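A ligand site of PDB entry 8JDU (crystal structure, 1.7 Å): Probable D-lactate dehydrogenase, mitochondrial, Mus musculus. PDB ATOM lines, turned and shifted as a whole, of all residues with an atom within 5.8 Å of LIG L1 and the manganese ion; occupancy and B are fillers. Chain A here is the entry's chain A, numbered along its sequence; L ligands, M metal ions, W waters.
Water W2 lies within hydrogen-bond range of an oxygen (O3) of LIG L1 (2.8 Å), the backbone NH (N) of Trp 338 (2.8 Å), the backbone carbonyl oxygen (O) of His 335 (2.8 Å) and the backbone NH (N) of Ala 337 (3.2 Å).
Water W1 lies within hydrogen-bond range of a ring nitrogen (ND1) of His 335, an oxygen (O3) of LIG L1, the backbone NH (N) of Gly 146 and the guanidinium group (NH1) of Arg 334.
O3 of LIG L1 lies within salt-bridge range of NH1 of Arg 334, 2.8 Å away.
An oxygen (O1) of LIG L1 lies close to a ring nitrogen (NE2) of His 430 (2.8 Å).
The side-chain carboxylate (OE2) of Glu 429 is in hydrogen-bond range of a nitrogen (N7) of LG2 L2, at 2.9 Å.
The backbone NH of Gly 146 lies within hydrogen-bond range of a nitrogen (N8) of LG2 L2 (3.1 Å).
An oxygen (O7) of LG2 L2 is in hydrogen-bond range of the backbone NH (N) of Ser 160 (3.1 Å).
The backbone carbonyl oxygen (O) of Ser 160 sits at hydrogen-bond distance from a nitrogen (N7) of LG2 L2 (3.1 Å).
Val 88 touches LIG L1.
Trp 338 touches LIG L1 (CE3 to C1, 3.6 Å).
OG of Ser 352 touches C2 of LIG L1, 3.7 Å away.
Within 4 Å of LIG L1: Val 88, Arg 334, Trp 338, Ser 352, His 385, His 392, Glu 429 and His 430.
The nearest printed residue that does not touch LIG L1 is His 335 (4.5 Å).
Within 4 Å of the manganese ion: His 385, His 392 and Glu 429.
The manganese ion is bound by OE1 of Glu 429 (2.1 Å).
An oxygen (O2) of LIG L1 binds the manganese ion (2.2 Å).
The manganese ion is bound by a ring nitrogen (NE2) of His 392.
The manganese ion is bound by an oxygen (O1) of LIG L1, at 2.5 Å.
The manganese ion is bound by NE2 of His 385 (2.5 Å).
The manganese ion has five donor atoms within binding distance.
Slightly farther from the manganese ion lies O8 of LG2 L2 (2.8 Å).
A ring nitrogen (NE2) of His 430 sits close to the side-chain carboxylate (OE1) of Glu 429 (3.4 Å).
N of Ser 160 sits close to OE2 of Glu 429, at 3.4 Å.
The backbone carbonyl oxygen (O) of Val 383 is in hydrogen-bond range of the backbone NH (N) of His 392 (2.7 Å).
A ring nitrogen (ND1) of His 392 lies close to the side-chain carboxylate of Asp 354, at 3.4 Å.
N of Asn 390 lies within hydrogen-bond range of O of His 385, at 3.3 Å.
The side-chain carboxylate of Glu 264 sits at hydrogen-bond distance from a ring nitrogen (ND1) of His 385, 2.8 Å away.
The side-chain carboxylate of Glu 264 is in salt-bridge range of the guanidinium group of Arg 334, at 2.8 Å.
N of His 430 is in hydrogen-bond range of OD2 of Asp 354.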
ATOM      1  N   VAL A  88      28.927  -8.257 -22.842  1.00  0.00           N
ATOM      2  CA  VAL A  88      28.752  -7.442 -21.645  1.00  0.00           C
ATOM      3  C   VAL A  88      30.032  -6.736 -21.226  1.00  0.00           C
ATOM      4  O   VAL A  88      30.158  -6.257 -20.111  1.00  0.00           O
ATOM      5  CB  VAL A  88      28.166  -8.261 -20.487  1.00  0.00           C
ATOM      6  CG1 VAL A  88      26.723  -8.651 -20.818  1.00  0.00           C
ATOM      7  CG2 VAL A  88      28.987  -9.489 -20.199  1.00  0.00           C
ATOM      8  N   GLY A 146      22.599 -17.080 -21.542  1.00  0.00           N
ATOM      9  CA  GLY A 146      21.211 -16.655 -21.387  1.00  0.00           C
ATOM     10  C   GLY A 146      20.655 -15.914 -22.578  1.00  0.00           C
ATOM     11  O   GLY A 146      19.455 -15.994 -22.869  1.00  0.00           O
ATOM     12  N   SER A 160      30.516 -19.603 -22.089  1.00  0.00           N
ATOM     13  CA  SER A 160      30.145 -20.805 -21.337  1.00  0.00           C
ATOM     14  C   SER A 160      28.642 -20.699 -21.114  1.00  0.00           C
ATOM     15  O   SER A 160      27.927 -19.954 -21.795  1.00  0.00           O
ATOM     16  CB  SER A 160      30.955 -20.894 -20.026  1.00  0.00           C
ATOM     17  OG  SER A 160      30.860 -22.166 -19.452  1.00  0.00           O
ATOM     18  N   GLY A 161      28.125 -21.445 -20.144  1.00  0.00           N
ATOM     19  CA  GLY A 161      26.699 -21.402 -19.861  1.00  0.00           C
ATOM     20  C   GLY A 161      26.398 -22.408 -18.789  1.00  0.00           C
ATOM     21  O   GLY A 161      27.302 -23.054 -18.244  1.00  0.00           O
ATOM     22  N   GLU A 264      23.351 -24.314 -10.714  1.00  0.00           N
ATOM     23  CA  GLU A 264      23.353 -22.864 -10.764  1.00  0.00           C
ATOM     24  C   GLU A 264      23.004 -22.295  -9.402  1.00  0.00           C
ATOM     25  O   GLU A 264      22.051 -22.747  -8.763  1.00  0.00           O
ATOM     26  CB  GLU A 264      22.364 -22.343 -11.777  1.00  0.00           C
ATOM     27  CG  GLU A 264      22.727 -22.647 -13.224  1.00  0.00           C
ATOM     28  CD  GLU A 264      23.974 -21.909 -13.667  1.00  0.00           C
ATOM     29  OE1 GLU A 264      24.966 -22.595 -14.037  1.00  0.00           O
ATOM     30  OE2 GLU A 264      23.999 -20.671 -13.538  1.00  0.00           O
ATOM     31  N   ARG A 334      16.181 -18.454 -15.197  1.00  0.00           N
ATOM     32  CA  ARG A 334      17.616 -18.345 -14.964  1.00  0.00           C
ATOM     33  C   ARG A 334      18.291 -17.600 -16.107  1.00  0.00           C
ATOM     34  O   ARG A 334      19.102 -16.698 -15.887  1.00  0.00           O
ATOM     35  CB  ARG A 334      18.219 -19.737 -14.758  1.00  0.00           C
ATOM     36  CG  ARG A 334      19.730 -19.804 -14.881  1.00  0.00           C
ATOM     37  CD  ARG A 334      20.391 -19.003 -13.774  1.00  0.00           C
ATOM     38  NE  ARG A 334      21.830 -18.957 -13.970  1.00  0.00           N
ATOM     39  CZ  ARG A 334      22.465 -17.996 -14.639  1.00  0.00           C
ATOM     40  NH1 ARG A 334      21.784 -16.969 -15.157  1.00  0.00           N
ATOM     41  NH2 ARG A 334      23.793 -18.056 -14.786  1.00  0.00           N
ATOM     42  N   HIS A 335      17.943 -17.961 -17.342  1.00  0.00           N
ATOM     43  CA  HIS A 335      18.579 -17.322 -18.494  1.00  0.00           C
ATOM     44  C   HIS A 335      18.281 -15.829 -18.542  1.00  0.00           C
ATOM     45  O   HIS A 335      19.077 -15.071 -19.121  1.00  0.00           O
ATOM     46  CB  HIS A 335      18.111 -17.978 -19.801  1.00  0.00           C
ATOM     47  CG  HIS A 335      18.747 -19.310 -20.072  1.00  0.00           C
ATOM     48  ND1 HIS A 335      20.031 -19.612 -19.685  1.00  0.00           N
ATOM     49  CD2 HIS A 335      18.274 -20.409 -20.699  1.00  0.00           C
ATOM     50  CE1 HIS A 335      20.323 -20.840 -20.068  1.00  0.00           C
ATOM     51  NE2 HIS A 335      19.274 -21.346 -20.689  1.00  0.00           N
ATOM     52  N   ALA A 337      18.106 -13.866 -15.838  1.00  0.00           N
ATOM     53  CA  ALA A 337      18.509 -13.251 -14.572  1.00  0.00           C
ATOM     54  C   ALA A 337      19.070 -11.847 -14.771  1.00  0.00           C
ATOM     55  O   ALA A 337      18.839 -10.948 -13.956  1.00  0.00           O
ATOM     56  CB  ALA A 337      19.535 -14.157 -13.875  1.00  0.00           C
ATOM     57  N   TRP A 338      19.845 -11.635 -15.839  1.00  0.00           N
ATOM     58  CA  TRP A 338      20.371 -10.304 -16.109  1.00  0.00           C
ATOM     59  C   TRP A 338      19.257  -9.266 -16.202  1.00  0.00           C
ATOM     60  O   TRP A 338      19.368  -8.173 -15.625  1.00  0.00           O
ATOM     61  CB  TRP A 338      21.196 -10.352 -17.396  1.00  0.00           C
ATOM     62  CG  TRP A 338      21.692  -9.048 -17.968  1.00  0.00           C
ATOM     63  CD1 TRP A 338      21.145  -8.356 -19.009  1.00  0.00           C
ATOM     64  CD2 TRP A 338      22.875  -8.332 -17.581  1.00  0.00           C
ATOM     65  NE1 TRP A 338      21.904  -7.248 -19.283  1.00  0.00           N
ATOM     66  CE2 TRP A 338      22.964  -7.206 -18.422  1.00  0.00           C
ATOM     67  CE3 TRP A 338      23.851  -8.528 -16.602  1.00  0.00           C
ATOM     68  CZ2 TRP A 338      23.989  -6.277 -18.318  1.00  0.00           C
ATOM     69  CZ3 TRP A 338      24.876  -7.599 -16.497  1.00  0.00           C
ATOM     70  CH2 TRP A 338      24.941  -6.494 -17.359  1.00  0.00           C
ATOM     71  N   SER A 352      28.546  -6.772 -14.830  1.00  0.00           N
ATOM     72  CA  SER A 352      28.697  -8.106 -14.273  1.00  0.00           C
ATOM     73  C   SER A 352      30.166  -8.395 -14.018  1.00  0.00           C
ATOM     74  O   SER A 352      31.004  -8.169 -14.901  1.00  0.00           O
ATOM     75  CB  SER A 352      28.111  -9.159 -15.209  1.00  0.00           C
ATOM     76  OG  SER A 352      28.210 -10.453 -14.619  1.00  0.00           O
ATOM     77  N   ASP A 354      32.770 -11.696 -13.148  1.00  0.00           N
ATOM     78  CA  ASP A 354      32.826 -13.004 -13.794  1.00  0.00           C
ATOM     79  C   ASP A 354      34.021 -13.837 -13.327  1.00  0.00           C
ATOM     80  O   ASP A 354      34.586 -14.608 -14.111  1.00  0.00           O
ATOM     81  CB  ASP A 354      32.867 -12.808 -15.315  1.00  0.00           C
ATOM     82  CG  ASP A 354      32.767 -14.116 -16.098  1.00  0.00           C
ATOM     83  OD1 ASP A 354      32.051 -15.050 -15.700  1.00  0.00           O
ATOM     84  OD2 ASP A 354      33.381 -14.174 -17.188  1.00  0.00           O
ATOM     85  N   VAL A 383      24.599 -14.648  -9.047  1.00  0.00           N
ATOM     86  CA  VAL A 383      24.088 -15.787  -9.793  1.00  0.00           C
ATOM     87  C   VAL A 383      25.287 -16.405 -10.490  1.00  0.00           C
ATOM     88  O   VAL A 383      26.250 -15.706 -10.818  1.00  0.00           O
ATOM     89  CB  VAL A 383      22.998 -15.339 -10.809  1.00  0.00           C
ATOM     90  CG1 VAL A 383      23.630 -14.419 -11.881  1.00  0.00           C
ATOM     91  CG2 VAL A 383      22.331 -16.522 -11.452  1.00  0.00           C
ATOM     92  N   GLY A 384      25.261 -17.717 -10.688  1.00  0.00           N
ATOM     93  CA  GLY A 384      26.251 -18.197 -11.646  1.00  0.00           C
ATOM     94  C   GLY A 384      26.578 -19.669 -11.594  1.00  0.00           C
ATOM     95  O   GLY A 384      25.993 -20.465 -10.854  1.00  0.00           O
ATOM     96  N   HIS A 385      27.564 -20.001 -12.444  1.00  0.00           N
ATOM     97  CA  HIS A 385      27.948 -21.361 -12.801  1.00  0.00           C
ATOM     98  C   HIS A 385      28.936 -21.881 -11.764  1.00  0.00           C
ATOM     99  O   HIS A 385      30.122 -22.124 -12.030  1.00  0.00           O
ATOM    100  CB  HIS A 385      28.547 -21.390 -14.204  1.00  0.00           C
ATOM    101  CG  HIS A 385      27.778 -20.566 -15.198  1.00  0.00           C
ATOM    102  ND1 HIS A 385      26.468 -20.827 -15.534  1.00  0.00           N
ATOM    103  CD2 HIS A 385      28.185 -19.552 -16.005  1.00  0.00           C
ATOM    104  CE1 HIS A 385      26.073 -19.974 -16.450  1.00  0.00           C
ATOM    105  NE2 HIS A 385      27.098 -19.192 -16.772  1.00  0.00           N
ATOM    106  N   ASN A 390      32.731 -20.547 -10.784  1.00  0.00           N
ATOM    107  CA  ASN A 390      32.506 -19.279 -11.459  1.00  0.00           C
ATOM    108  C   ASN A 390      31.193 -18.685 -10.950  1.00  0.00           C
ATOM    109  O   ASN A 390      30.268 -19.414 -10.610  1.00  0.00           O
ATOM    110  CB  ASN A 390      32.480 -19.569 -12.988  1.00  0.00           C
ATOM    111  CG  ASN A 390      32.041 -18.393 -13.868  1.00  0.00           C
ATOM    112  OD1 ASN A 390      31.154 -18.555 -14.708  1.00  0.00           O
ATOM    113  ND2 ASN A 390      32.680 -17.245 -13.708  1.00  0.00           N
ATOM    114  N   HIS A 392      28.700 -14.652 -11.070  1.00  0.00           N
ATOM    115  CA  HIS A 392      28.528 -13.268 -11.484  1.00  0.00           C
ATOM    116  C   HIS A 392      27.962 -12.444 -10.331  1.00  0.00           C
ATOM    117  O   HIS A 392      26.971 -12.852  -9.703  1.00  0.00           O
ATOM    118  CB  HIS A 392      27.564 -13.139 -12.672  1.00  0.00           C
ATOM    119  CG  HIS A 392      27.883 -14.050 -13.806  1.00  0.00           C
ATOM    120  ND1 HIS A 392      29.070 -13.987 -14.496  1.00  0.00           N
ATOM    121  CD2 HIS A 392      27.157 -15.043 -14.378  1.00  0.00           C
ATOM    122  CE1 HIS A 392      29.069 -14.903 -15.445  1.00  0.00           C
ATOM    123  NE2 HIS A 392      27.928 -15.565 -15.395  1.00  0.00           N
ATOM    124  N   ILE A 394      26.080  -9.112 -10.287  1.00  0.00           N
ATOM    125  CA  ILE A 394      25.441  -8.154 -11.189  1.00  0.00           C
ATOM    126  C   ILE A 394      25.186  -6.887 -10.401  1.00  0.00           C
ATOM    127  O   ILE A 394      24.385  -6.885  -9.463  1.00  0.00           O
ATOM    128  CB  ILE A 394      24.133  -8.717 -11.759  1.00  0.00           C
ATOM    129  CG1 ILE A 394      24.388  -9.986 -12.571  1.00  0.00           C
ATOM    130  CG2 ILE A 394      23.462  -7.673 -12.642  1.00  0.00           C
ATOM    131  CD1 ILE A 394      23.103 -10.685 -13.012  1.00  0.00           C
ATOM    132  N   GLU A 429      34.153 -16.470 -18.569  1.00  0.00           N
ATOM    133  CA  GLU A 429      33.475 -16.642 -19.854  1.00  0.00           C
ATOM    134  C   GLU A 429      33.174 -15.360 -20.624  1.00  0.00           C
ATOM    135  O   GLU A 429      33.083 -15.400 -21.852  1.00  0.00           O
ATOM    136  CB  GLU A 429      32.155 -17.394 -19.639  1.00  0.00           C
ATOM    137  CG  GLU A 429      31.287 -16.703 -18.598  1.00  0.00           C
ATOM    138  CD  GLU A 429      29.868 -17.253 -18.547  1.00  0.00           C
ATOM    139  OE1 GLU A 429      29.001 -16.564 -17.984  1.00  0.00           O
ATOM    140  OE2 GLU A 429      29.619 -18.378 -19.046  1.00  0.00           O
ATOM    141  N   HIS A 430      32.969 -14.227 -19.926  1.00  0.00           N
ATOM    142  CA  HIS A 430      32.512 -13.028 -20.628  1.00  0.00           C
ATOM    143  C   HIS A 430      33.598 -12.372 -21.465  1.00  0.00           C
ATOM    144  O   HIS A 430      33.278 -11.739 -22.473  1.00  0.00           O
ATOM    145  CB  HIS A 430      32.003 -11.974 -19.647  1.00  0.00           C
ATOM    146  CG  HIS A 430      30.722 -12.345 -18.987  1.00  0.00           C
ATOM    147  ND1 HIS A 430      30.297 -11.740 -17.826  1.00  0.00           N
ATOM    148  CD2 HIS A 430      29.765 -13.253 -19.315  1.00  0.00           C
ATOM    149  CE1 HIS A 430      29.126 -12.251 -17.462  1.00  0.00           C
ATOM    150  NE2 HIS A 430      28.793 -13.178 -18.350  1.00  0.00           N
HETATM  151  C1  LIG L   1      25.301 -11.239 -18.463  1.00  0.00           C
HETATM  152  C2  LIG L   1      25.687 -11.679 -17.049  1.00  0.00           C
HETATM  153  C3  LIG L   1      24.782 -12.853 -16.666  1.00  0.00           C
HETATM  154  C4  LIG L   1      25.255 -14.204 -17.212  1.00  0.00           C
HETATM  155  O1  LIG L   1      26.277 -14.392 -17.802  1.00  0.00           O
HETATM  156  C5  LIG L   1      24.360 -15.384 -16.944  1.00  0.00           C
HETATM  157  O2  LIG L   1      24.903 -16.465 -16.645  1.00  0.00           O
HETATM  158  O3  LIG L   1      23.096 -15.274 -17.030  1.00  0.00           O
HETATM  159  P1  LG2 L   2      28.868  -9.170 -29.647  1.00  0.00           P
HETATM  160  O1  LG2 L   2      28.285  -8.894 -30.967  1.00  0.00           O
HETATM  161  O2  LG2 L   2      28.473  -8.261 -28.488  1.00  0.00           O
HETATM  162  O3  LG2 L   2      30.454  -9.210 -29.736  1.00  0.00           O
HETATM  163  C1  LG2 L   2      31.234  -9.653 -28.601  1.00  0.00           C
HETATM  164  C2  LG2 L   2      32.708  -9.550 -28.917  1.00  0.00           C
HETATM  165  O4  LG2 L   2      33.055 -10.581 -29.864  1.00  0.00           O
HETATM  166  C3  LG2 L   2      33.144  -8.232 -29.558  1.00  0.00           C
HETATM  167  O5  LG2 L   2      34.473  -7.905 -29.163  1.00  0.00           O
HETATM  168  C4  LG2 L   2      33.047  -8.525 -31.052  1.00  0.00           C
HETATM  169  O6  LG2 L   2      33.952  -7.738 -31.833  1.00  0.00           O
HETATM  170  C5  LG2 L   2      33.448 -10.005 -31.096  1.00  0.00           C
HETATM  171  N1  LG2 L   2      32.810 -10.770 -32.159  1.00  0.00           N
HETATM  172  C6  LG2 L   2      31.471 -11.016 -32.345  1.00  0.00           C
HETATM  173  N2  LG2 L   2      31.207 -11.782 -33.377  1.00  0.00           N
HETATM  174  C7  LG2 L   2      32.466 -12.062 -33.905  1.00  0.00           C
HETATM  175  C8  LG2 L   2      32.884 -12.800 -35.022  1.00  0.00           C
HETATM  176  N3  LG2 L   2      32.049 -13.459 -35.828  1.00  0.00           N
HETATM  177  N4  LG2 L   2      34.221 -12.872 -35.270  1.00  0.00           N
HETATM  178  C9  LG2 L   2      35.054 -12.234 -34.451  1.00  0.00           C
HETATM  179  N5  LG2 L   2      34.772 -11.490 -33.386  1.00  0.00           N
HETATM  180  C10 LG2 L   2      33.458 -11.442 -33.165  1.00  0.00           C
HETATM  181  N6  LG2 L   2      28.020 -15.027 -21.954  1.00  0.00           N
HETATM  182  C11 LG2 L   2      28.470 -16.231 -21.510  1.00  0.00           C
HETATM  183  O7  LG2 L   2      29.596 -16.671 -21.793  1.00  0.00           O
HETATM  184  N7  LG2 L   2      27.646 -17.036 -20.733  1.00  0.00           N
HETATM  185  C12 LG2 L   2      26.359 -16.725 -20.319  1.00  0.00           C
HETATM  186  O8  LG2 L   2      25.741 -17.514 -19.617  1.00  0.00           O
HETATM  187  C13 LG2 L   2      25.884 -15.443 -20.797  1.00  0.00           C
HETATM  188  N8  LG2 L   2      24.661 -15.068 -20.473  1.00  0.00           N
HETATM  189  C14 LG2 L   2      24.211 -13.850 -20.918  1.00  0.00           C
HETATM  190  C15 LG2 L   2      22.914 -13.450 -20.595  1.00  0.00           C
HETATM  191  C16 LG2 L   2      22.413 -12.229 -21.041  1.00  0.00           C
HETATM  192  C17 LG2 L   2      21.015 -11.815 -20.653  1.00  0.00           C
HETATM  193  C18 LG2 L   2      23.221 -11.381 -21.821  1.00  0.00           C
HETATM  194  C19 LG2 L   2      22.720 -10.049 -22.306  1.00  0.00           C
HETATM  195  C20 LG2 L   2      24.513 -11.789 -22.165  1.00  0.00           C
HETATM  196  C21 LG2 L   2      25.004 -13.002 -21.723  1.00  0.00           C
HETATM  197  N9  LG2 L   2      26.305 -13.445 -22.060  1.00  0.00           N
HETATM  198  C22 LG2 L   2      26.784 -14.657 -21.610  1.00  0.00           C
HETATM  199  C23 LG2 L   2      27.208 -12.566 -22.841  1.00  0.00           C
HETATM  200  C24 LG2 L   2      27.084 -12.710 -24.357  1.00  0.00           C
HETATM  201  O9  LG2 L   2      25.824 -13.272 -24.709  1.00  0.00           O
HETATM  202  C25 LG2 L   2      28.187 -13.627 -24.879  1.00  0.00           C
HETATM  203  O10 LG2 L   2      29.431 -13.030 -24.541  1.00  0.00           O
HETATM  204  C26 LG2 L   2      28.097 -13.899 -26.379  1.00  0.00           C
HETATM  205  O11 LG2 L   2      29.098 -14.860 -26.715  1.00  0.00           O
HETATM  206  C27 LG2 L   2      28.266 -12.642 -27.202  1.00  0.00           C
HETATM  207  O12 LG2 L   2      27.939 -12.919 -28.584  1.00  0.00           O
HETATM  208  P2  LG2 L   2      27.485 -11.760 -29.537  1.00  0.00           P
HETATM  209  O13 LG2 L   2      27.544 -12.172 -31.012  1.00  0.00           O
HETATM  210  O14 LG2 L   2      26.135 -11.222 -29.051  1.00  0.00           O
HETATM  211  O15 LG2 L   2      28.606 -10.683 -29.224  1.00  0.00           O
HETATM  212 MN    MN M   1      26.976 -16.737 -17.285  1.00  0.00          MN
HETATM  213  O   HOH W   1      22.138 -17.779 -18.475  1.00  0.00           O
HETATM  214  O   HOH W   2      20.883 -13.651 -17.480  1.00  0.00           O
